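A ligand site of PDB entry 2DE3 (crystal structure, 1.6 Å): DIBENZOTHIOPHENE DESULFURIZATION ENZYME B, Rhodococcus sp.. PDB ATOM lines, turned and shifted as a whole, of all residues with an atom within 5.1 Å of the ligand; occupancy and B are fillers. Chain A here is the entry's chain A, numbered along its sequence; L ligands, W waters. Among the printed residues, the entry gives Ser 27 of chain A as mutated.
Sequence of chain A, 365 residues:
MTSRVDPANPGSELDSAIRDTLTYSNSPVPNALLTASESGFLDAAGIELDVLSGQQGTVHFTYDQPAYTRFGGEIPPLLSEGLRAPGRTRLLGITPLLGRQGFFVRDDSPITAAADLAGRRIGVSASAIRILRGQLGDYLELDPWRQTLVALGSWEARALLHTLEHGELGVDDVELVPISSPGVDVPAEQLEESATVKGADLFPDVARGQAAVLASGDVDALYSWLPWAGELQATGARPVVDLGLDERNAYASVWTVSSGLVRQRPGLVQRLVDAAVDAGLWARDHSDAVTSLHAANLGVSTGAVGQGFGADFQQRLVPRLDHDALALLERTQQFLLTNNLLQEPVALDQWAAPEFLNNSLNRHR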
ATOM      1  N   ASN A  26      31.967   6.973 -29.257  1.00  0.00           N
ATOM      2  CA  ASN A  26      30.551   6.945 -28.902  1.00  0.00           C
ATOM      3  C   ASN A  26      29.868   5.861 -29.711  1.00  0.00           C
ATOM      4  O   ASN A  26      30.289   5.536 -30.826  1.00  0.00           O
ATOM      5  CB  ASN A  26      29.857   8.302 -29.130  1.00  0.00           C
ATOM      6  CG  ASN A  26      29.916   8.789 -30.567  1.00  0.00           C
ATOM      7  OD1 ASN A  26      30.870   9.467 -30.971  1.00  0.00           O
ATOM      8  ND2 ASN A  26      28.890   8.469 -31.354  1.00  0.00           N
ATOM      9  N   SER A  27      28.831   5.265 -29.125  1.00  0.00           N
ATOM     10  CA  SER A  27      28.061   4.221 -29.792  1.00  0.00           C
ATOM     11  C   SER A  27      27.065   4.916 -30.702  1.00  0.00           C
ATOM     12  O   SER A  27      26.969   6.141 -30.707  1.00  0.00           O
ATOM     13  CB  SER A  27      27.309   3.392 -28.748  1.00  0.00           C
ATOM     14  OG  SER A  27      28.187   2.772 -27.828  1.00  0.00           O
ATOM     15  N   PRO A  28      26.308   4.144 -31.511  1.00  0.00           N
ATOM     16  CA  PRO A  28      25.320   4.737 -32.414  1.00  0.00           C
ATOM     17  C   PRO A  28      24.059   5.120 -31.636  1.00  0.00           C
ATOM     18  O   PRO A  28      22.963   4.590 -31.877  1.00  0.00           O
ATOM     19  CB  PRO A  28      25.050   3.627 -33.431  1.00  0.00           C
ATOM     20  CG  PRO A  28      26.275   2.725 -33.328  1.00  0.00           C
ATOM     21  CD  PRO A  28      26.551   2.728 -31.851  1.00  0.00           C
ATOM     22  N   VAL A  29      24.218   6.052 -30.694  1.00  0.00           N
ATOM     23  CA  VAL A  29      23.135   6.519 -29.841  1.00  0.00           C
ATOM     24  C   VAL A  29      23.168   8.051 -29.715  1.00  0.00           C
ATOM     25  O   VAL A  29      24.204   8.673 -29.954  1.00  0.00           O
ATOM     26  CB  VAL A  29      23.263   5.901 -28.426  1.00  0.00           C
ATOM     27  CG1 VAL A  29      23.344   4.390 -28.516  1.00  0.00           C
ATOM     28  CG2 VAL A  29      24.508   6.457 -27.726  1.00  0.00           C
ATOM     29  N   HIS A  60      37.131   0.651 -26.356  1.00  0.00           N
ATOM     30  CA  HIS A  60      35.703   0.961 -26.346  1.00  0.00           C
ATOM     31  C   HIS A  60      35.002  -0.005 -25.383  1.00  0.00           C
ATOM     32  O   HIS A  60      33.919   0.298 -24.849  1.00  0.00           O
ATOM     33  CB  HIS A  60      35.157   0.791 -27.782  1.00  0.00           C
ATOM     34  CG  HIS A  60      33.725   1.233 -27.966  1.00  0.00           C
ATOM     35  ND1 HIS A  60      33.357   2.562 -28.007  1.00  0.00           N
ATOM     36  CD2 HIS A  60      32.599   0.519 -28.162  1.00  0.00           C
ATOM     37  CE1 HIS A  60      32.064   2.645 -28.247  1.00  0.00           C
ATOM     38  NE2 HIS A  60      31.569   1.423 -28.336  1.00  0.00           N
ATOM     39  N   PHE A  61      35.621  -1.171 -25.140  1.00  0.00           N
ATOM     40  CA  PHE A  61      35.084  -2.196 -24.237  1.00  0.00           C
ATOM     41  C   PHE A  61      35.911  -2.371 -22.958  1.00  0.00           C
ATOM     42  O   PHE A  61      35.394  -2.869 -21.956  1.00  0.00           O
ATOM     43  CB  PHE A  61      35.047  -3.576 -24.927  1.00  0.00           C
ATOM     44  CG  PHE A  61      33.915  -3.777 -25.916  1.00  0.00           C
ATOM     45  CD1 PHE A  61      33.090  -2.729 -26.316  1.00  0.00           C
ATOM     46  CD2 PHE A  61      33.720  -5.042 -26.489  1.00  0.00           C
ATOM     47  CE1 PHE A  61      32.082  -2.937 -27.261  1.00  0.00           C
ATOM     48  CE2 PHE A  61      32.722  -5.260 -27.432  1.00  0.00           C
ATOM     49  CZ  PHE A  61      31.898  -4.209 -27.822  1.00  0.00           C
ATOM     50  N   ARG A  70      33.940   8.032 -23.048  1.00  0.00           N
ATOM     51  CA  ARG A  70      33.006   7.354 -23.961  1.00  0.00           C
ATOM     52  C   ARG A  70      31.557   7.620 -23.592  1.00  0.00           C
ATOM     53  O   ARG A  70      31.227   7.725 -22.413  1.00  0.00           O
ATOM     54  CB  ARG A  70      33.258   5.837 -23.929  1.00  0.00           C
ATOM     55  CG  ARG A  70      32.197   4.947 -24.634  1.00  0.00           C
ATOM     56  CD  ARG A  70      32.544   3.467 -24.434  1.00  0.00           C
ATOM     57  NE  ARG A  70      31.629   2.500 -25.047  1.00  0.00           N
ATOM     58  CZ  ARG A  70      30.417   2.199 -24.591  1.00  0.00           C
ATOM     59  NH1 ARG A  70      29.939   2.796 -23.507  1.00  0.00           N
ATOM     60  NH2 ARG A  70      29.694   1.266 -25.200  1.00  0.00           N
ATOM     61  N   GLY A  72      28.107   5.830 -24.660  1.00  0.00           N
ATOM     62  CA  GLY A  72      27.486   4.782 -25.455  1.00  0.00           C
ATOM     63  C   GLY A  72      26.669   3.757 -24.662  1.00  0.00           C
ATOM     64  O   GLY A  72      26.217   4.041 -23.544  1.00  0.00           O
ATOM     65  N   GLY A  73      26.473   2.588 -25.263  1.00  0.00           N
ATOM     66  CA  GLY A  73      25.703   1.531 -24.622  1.00  0.00           C
ATOM     67  C   GLY A  73      26.263   1.161 -23.253  1.00  0.00           C
ATOM     68  O   GLY A  73      27.474   1.180 -23.055  1.00  0.00           O
ATOM     69  N   GLU A  74      25.380   0.806 -22.332  1.00  0.00           N
ATOM     70  CA  GLU A  74      25.800   0.488 -20.965  1.00  0.00           C
ATOM     71  C   GLU A  74      26.356  -0.909 -20.692  1.00  0.00           C
ATOM     72  O   GLU A  74      26.973  -1.129 -19.642  1.00  0.00           O
ATOM     73  CB  GLU A  74      24.643   0.739 -19.992  1.00  0.00           C
ATOM     74  CG  GLU A  74      23.434  -0.218 -20.164  1.00  0.00           C
ATOM     75  CD  GLU A  74      22.327   0.349 -21.049  1.00  0.00           C
ATOM     76  OE1 GLU A  74      22.608   0.729 -22.205  1.00  0.00           O
ATOM     77  OE2 GLU A  74      21.173   0.404 -20.584  1.00  0.00           O
ATOM     78  N   ILE A  75      26.160  -1.852 -21.596  1.00  0.00           N
ATOM     79  CA  ILE A  75      26.637  -3.199 -21.331  1.00  0.00           C
ATOM     80  C   ILE A  75      28.159  -3.339 -21.220  1.00  0.00           C
ATOM     81  O   ILE A  75      28.648  -3.951 -20.267  1.00  0.00           O
ATOM     82  CB  ILE A  75      26.048  -4.206 -22.348  1.00  0.00           C
ATOM     83  CG1 ILE A  75      24.524  -4.223 -22.205  1.00  0.00           C
ATOM     84  CG2 ILE A  75      26.601  -5.611 -22.104  1.00  0.00           C
ATOM     85  CD1 ILE A  75      23.798  -5.132 -23.207  1.00  0.00           C
ATOM     86  N   PRO A  76      28.933  -2.784 -22.167  1.00  0.00           N
ATOM     87  CA  PRO A  76      30.387  -2.929 -22.039  1.00  0.00           C
ATOM     88  C   PRO A  76      30.961  -2.349 -20.732  1.00  0.00           C
ATOM     89  O   PRO A  76      31.758  -3.007 -20.054  1.00  0.00           O
ATOM     90  CB  PRO A  76      30.917  -2.234 -23.296  1.00  0.00           C
ATOM     91  CG  PRO A  76      29.822  -2.511 -24.297  1.00  0.00           C
ATOM     92  CD  PRO A  76      28.572  -2.244 -23.488  1.00  0.00           C
ATOM     93  N   TRP A 145      37.031  -8.638 -25.393  1.00  0.00           N
ATOM     94  CA  TRP A 145      36.254  -8.335 -26.588  1.00  0.00           C
ATOM     95  C   TRP A 145      35.182  -9.381 -26.893  1.00  0.00           C
ATOM     96  O   TRP A 145      34.004  -9.046 -27.017  1.00  0.00           O
ATOM     97  CB  TRP A 145      37.179  -8.145 -27.800  1.00  0.00           C
ATOM     98  CG  TRP A 145      36.466  -7.574 -29.003  1.00  0.00           C
ATOM     99  CD1 TRP A 145      35.999  -8.258 -30.092  1.00  0.00           C
ATOM    100  CD2 TRP A 145      36.096  -6.207 -29.201  1.00  0.00           C
ATOM    101  NE1 TRP A 145      35.352  -7.400 -30.945  1.00  0.00           N
ATOM    102  CE2 TRP A 145      35.392  -6.129 -30.422  1.00  0.00           C
ATOM    103  CE3 TRP A 145      36.274  -5.029 -28.456  1.00  0.00           C
ATOM    104  CZ2 TRP A 145      34.873  -4.932 -30.923  1.00  0.00           C
ATOM    105  CZ3 TRP A 145      35.765  -3.832 -28.958  1.00  0.00           C
ATOM    106  CH2 TRP A 145      35.060  -3.795 -30.177  1.00  0.00           C
ATOM    107  N   LEU A 149      30.895  -9.264 -26.465  1.00  0.00           N
ATOM    108  CA  LEU A 149      30.020  -9.537 -27.602  1.00  0.00           C
ATOM    109  C   LEU A 149      28.942 -10.561 -27.277  1.00  0.00           C
ATOM    110  O   LEU A 149      27.841 -10.527 -27.844  1.00  0.00           O
ATOM    111  CB  LEU A 149      30.841  -9.984 -28.823  1.00  0.00           C
ATOM    112  CG  LEU A 149      31.743  -8.911 -29.449  1.00  0.00           C
ATOM    113  CD1 LEU A 149      32.441  -9.513 -30.666  1.00  0.00           C
ATOM    114  CD2 LEU A 149      30.932  -7.686 -29.848  1.00  0.00           C
ATOM    115  N   LEU A 152      26.227  -8.675 -25.542  1.00  0.00           N
ATOM    116  CA  LEU A 152      25.460  -7.779 -26.405  1.00  0.00           C
ATOM    117  C   LEU A 152      24.285  -8.519 -27.059  1.00  0.00           C
ATOM    118  O   LEU A 152      23.421  -7.909 -27.686  1.00  0.00           O
ATOM    119  CB  LEU A 152      26.356  -7.142 -27.470  1.00  0.00           C
ATOM    120  CG  LEU A 152      27.455  -6.198 -26.940  1.00  0.00           C
ATOM    121  CD1 LEU A 152      28.084  -5.436 -28.110  1.00  0.00           C
ATOM    122  CD2 LEU A 152      26.858  -5.196 -25.928  1.00  0.00           C
ATOM    123  N   TRP A 155      20.204  -7.528 -26.302  1.00  0.00           N
ATOM    124  CA  TRP A 155      19.208  -6.700 -27.000  1.00  0.00           C
ATOM    125  C   TRP A 155      18.176  -7.571 -27.713  1.00  0.00           C
ATOM    126  O   TRP A 155      16.967  -7.370 -27.577  1.00  0.00           O
ATOM    127  CB  TRP A 155      19.883  -5.772 -28.023  1.00  0.00           C
ATOM    128  CG  TRP A 155      21.001  -4.898 -27.485  1.00  0.00           C
ATOM    129  CD1 TRP A 155      21.016  -4.198 -26.298  1.00  0.00           C
ATOM    130  CD2 TRP A 155      22.216  -4.575 -28.157  1.00  0.00           C
ATOM    131  NE1 TRP A 155      22.183  -3.471 -26.203  1.00  0.00           N
ATOM    132  CE2 TRP A 155      22.937  -3.683 -27.327  1.00  0.00           C
ATOM    133  CE3 TRP A 155      22.776  -4.962 -29.381  1.00  0.00           C
ATOM    134  CZ2 TRP A 155      24.181  -3.159 -27.693  1.00  0.00           C
ATOM    135  CZ3 TRP A 155      24.021  -4.438 -29.747  1.00  0.00           C
ATOM    136  CH2 TRP A 155      24.713  -3.542 -28.905  1.00  0.00           C
ATOM    137  N   GLY A 183      26.777  -4.982 -34.527  1.00  0.00           N
ATOM    138  CA  GLY A 183      27.209  -4.631 -33.184  1.00  0.00           C
ATOM    139  C   GLY A 183      27.489  -5.849 -32.311  1.00  0.00           C
ATOM    140  O   GLY A 183      28.235  -5.758 -31.340  1.00  0.00           O
ATOM    141  N   VAL A 186      31.172  -8.733 -34.466  1.00  0.00           N
ATOM    142  CA  VAL A 186      32.251  -7.843 -34.858  1.00  0.00           C
ATOM    143  C   VAL A 186      33.603  -8.517 -34.612  1.00  0.00           C
ATOM    144  O   VAL A 186      34.189  -8.386 -33.533  1.00  0.00           O
ATOM    145  CB  VAL A 186      32.216  -6.523 -34.050  1.00  0.00           C
ATOM    146  CG1 VAL A 186      33.286  -5.554 -34.568  1.00  0.00           C
ATOM    147  CG2 VAL A 186      30.836  -5.890 -34.146  1.00  0.00           C
ATOM    148  N   LEU A 202      32.760   1.383 -38.803  1.00  0.00           N
ATOM    149  CA  LEU A 202      32.567   0.046 -38.271  1.00  0.00           C
ATOM    150  C   LEU A 202      31.280  -0.663 -38.705  1.00  0.00           C
ATOM    151  O   LEU A 202      31.252  -1.890 -38.855  1.00  0.00           O
ATOM    152  CB  LEU A 202      32.627   0.106 -36.739  1.00  0.00           C
ATOM    153  CG  LEU A 202      32.858  -1.176 -35.948  1.00  0.00           C
ATOM    154  CD1 LEU A 202      34.138  -1.860 -36.433  1.00  0.00           C
ATOM    155  CD2 LEU A 202      32.971  -0.830 -34.470  1.00  0.00           C
ATOM    156  N   PHE A 203      30.224   0.114 -38.923  1.00  0.00           N
ATOM    157  CA  PHE A 203      28.926  -0.452 -39.292  1.00  0.00           C
ATOM    158  C   PHE A 203      28.337   0.126 -40.582  1.00  0.00           C
ATOM    159  O   PHE A 203      27.257   0.722 -40.559  1.00  0.00           O
ATOM    160  CB  PHE A 203      27.923  -0.238 -38.156  1.00  0.00           C
ATOM    161  CG  PHE A 203      28.428  -0.699 -36.819  1.00  0.00           C
ATOM    162  CD1 PHE A 203      28.731  -2.037 -36.592  1.00  0.00           C
ATOM    163  CD2 PHE A 203      28.595   0.210 -35.777  1.00  0.00           C
ATOM    164  CE1 PHE A 203      29.208  -2.465 -35.356  1.00  0.00           C
ATOM    165  CE2 PHE A 203      29.073  -0.215 -34.531  1.00  0.00           C
ATOM    166  CZ  PHE A 203      29.374  -1.549 -34.327  1.00  0.00           C
ATOM    167  N   TRP A 225      17.048  -2.054 -34.789  1.00  0.00           N
ATOM    168  CA  TRP A 225      16.781  -0.875 -33.962  1.00  0.00           C
ATOM    169  C   TRP A 225      17.765   0.224 -34.352  1.00  0.00           C
ATOM    170  O   TRP A 225      18.523   0.068 -35.315  1.00  0.00           O
ATOM    171  CB  TRP A 225      16.910  -1.251 -32.469  1.00  0.00           C
ATOM    172  CG  TRP A 225      18.306  -1.648 -32.013  1.00  0.00           C
ATOM    173  CD1 TRP A 225      19.255  -2.316 -32.734  1.00  0.00           C
ATOM    174  CD2 TRP A 225      18.892  -1.384 -30.722  1.00  0.00           C
ATOM    175  NE1 TRP A 225      20.400  -2.483 -31.976  1.00  0.00           N
ATOM    176  CE2 TRP A 225      20.195  -1.925 -30.739  1.00  0.00           C
ATOM    177  CE3 TRP A 225      18.432  -0.754 -29.555  1.00  0.00           C
ATOM    178  CZ2 TRP A 225      21.062  -1.850 -29.639  1.00  0.00           C
ATOM    179  CZ3 TRP A 225      19.300  -0.669 -28.458  1.00  0.00           C
ATOM    180  CH2 TRP A 225      20.589  -1.220 -28.512  1.00  0.00           C
ATOM    181  N   LEU A 226      17.749   1.344 -33.625  1.00  0.00           N
ATOM    182  CA  LEU A 226      18.631   2.479 -33.922  1.00  0.00           C
ATOM    183  C   LEU A 226      18.291   2.994 -35.331  1.00  0.00           C
ATOM    184  O   LEU A 226      17.252   2.623 -35.894  1.00  0.00           O
ATOM    185  CB  LEU A 226      20.096   2.034 -33.824  1.00  0.00           C
ATOM    186  CG  LEU A 226      20.468   1.262 -32.554  1.00  0.00           C
ATOM    187  CD1 LEU A 226      21.970   0.961 -32.532  1.00  0.00           C
ATOM    188  CD2 LEU A 226      20.068   2.068 -31.317  1.00  0.00           C
ATOM    189  N   TRP A 228      19.415   2.125 -37.972  1.00  0.00           N
ATOM    190  CA  TRP A 228      19.435   0.974 -38.879  1.00  0.00           C
ATOM    191  C   TRP A 228      18.007   0.508 -39.150  1.00  0.00           C
ATOM    192  O   TRP A 228      17.663   0.136 -40.275  1.00  0.00           O
ATOM    193  CB  TRP A 228      20.266  -0.160 -38.268  1.00  0.00           C
ATOM    194  CG  TRP A 228      21.671   0.232 -37.890  1.00  0.00           C
ATOM    195  CD1 TRP A 228      22.459   1.144 -38.533  1.00  0.00           C
ATOM    196  CD2 TRP A 228      22.463  -0.306 -36.829  1.00  0.00           C
ATOM    197  NE1 TRP A 228      23.705   1.204 -37.933  1.00  0.00           N
ATOM    198  CE2 TRP A 228      23.725   0.315 -36.889  1.00  0.00           C
ATOM    199  CE3 TRP A 228      22.236  -1.273 -35.835  1.00  0.00           C
ATOM    200  CZ2 TRP A 228      24.760   0.024 -35.983  1.00  0.00           C
ATOM    201  CZ3 TRP A 228      23.249  -1.578 -34.943  1.00  0.00           C
ATOM    202  CH2 TRP A 228      24.500  -0.930 -35.021  1.00  0.00           C
HETATM  203  C1  LIG L   1      26.471  -0.817 -31.339  1.00  0.00           C
HETATM  204  C2  LIG L   1      27.351  -0.949 -30.276  1.00  0.00           C
HETATM  205  C3  LIG L   1      26.925  -0.626 -28.983  1.00  0.00           C
HETATM  206  C4  LIG L   1      25.626  -0.159 -28.789  1.00  0.00           C
HETATM  207  C5  LIG L   1      24.756  -0.018 -29.856  1.00  0.00           C
HETATM  208  C6  LIG L   1      25.172  -0.350 -31.145  1.00  0.00           C
HETATM  209  C7  LIG L   1      28.646  -1.388 -30.519  1.00  0.00           C
HETATM  210  C8  LIG L   1      28.918  -2.752 -30.532  1.00  0.00           C
HETATM  211  C9  LIG L   1      30.211  -3.218 -30.799  1.00  0.00           C
HETATM  212  C10 LIG L   1      31.234  -2.315 -31.033  1.00  0.00           C
HETATM  213  C11 LIG L   1      30.972  -0.941 -31.023  1.00  0.00           C
HETATM  214  C12 LIG L   1      29.688  -0.487 -30.764  1.00  0.00           C
HETATM  215  O1  LIG L   1      29.447   0.860 -30.739  1.00  0.00           O
HETATM  216  S1  LIG L   1      27.971  -0.843 -27.597  1.00  0.00           S
HETATM  217  O2  LIG L   1      29.031   0.112 -27.651  1.00  0.00           O
HETATM  218  O3  LIG L   1      27.189  -0.643 -26.331  1.00  0.00           O
HETATM  219  O   HOH W   1      25.463  -1.765 -24.511  1.00  0.00           O
HETATM  220  O   HOH W   2      31.140   2.933 -31.991  1.00  0.00           O
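NH2 of Arg 70 lies within salt-bridge range of O2 of the ligand (2.8 Å). A ring nitrogen (NE2) of His 60 is in hydrogen-bond range of an oxygen (O2) of the ligand, 2.9 Å away. N of Gly 73 sits close to O3 of the ligand. OG of Ser 27 lies within hydrogen-bond range of O2 of the ligand (2.8 Å).
OG of Ser 27 is in hydrogen-bond range of NH2 of Arg 70. The backbone carbonyl oxygen of Gly 73 sits at hydrogen-bond distance from the guanidinium group of Arg 70 (3.0 Å). The backbone carbonyl oxygen (O) of His 60 is in hydrogen-bond range of the guanidinium group (NE) of Arg 70, at 3.2 Å. The backbone NH of Gly 73 lies within hydrogen-bond range of the side-chain hydroxyl of Ser 27.
Residues that only touch the ligand: Pro 28 (3.4 Å), Phe 61 (3.6 Å), Pro 76 (3.5 Å), Leu 152 (3.7 Å), Trp 155 (3.5 Å), Gly 183 (3.2 Å), Leu 202 (3.99 Å), Phe 203 (3.7 Å), Leu 226 (3.7 Å) and Trp 228 (3.98 Å). Hydrophobic or aromatic side chains within 4 Å of the ligand: Pro 28, His 60, Phe 61, Pro 76, Leu 152, Trp 155, Leu 202, Phe 203, Leu 226 and Trp 228. 14 residues have an atom within 4 Å of the ligand: Ser 27, Pro 28, His 60, Phe 61, Arg 70, Gly 73, Pro 76, Leu 152, Trp 155, Gly 183, Leu 202, Phe 203, Leu 226 and Trp 228. Along chain A the residues within 4 Å of the ligand span positions 27 to 228.
Water W1 lies within hydrogen-bond range of an oxygen (O3) of the ligand (2.7 Å), the backbone NH (N) of Ile 75 (3.0 Å) and the backbone NH (N) of Glu 74 (3.4 Å). Water W2 lies within hydrogen-bond range of an oxygen (O1) of the ligand and the backbone carbonyl oxygen (O) of Asn 26.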
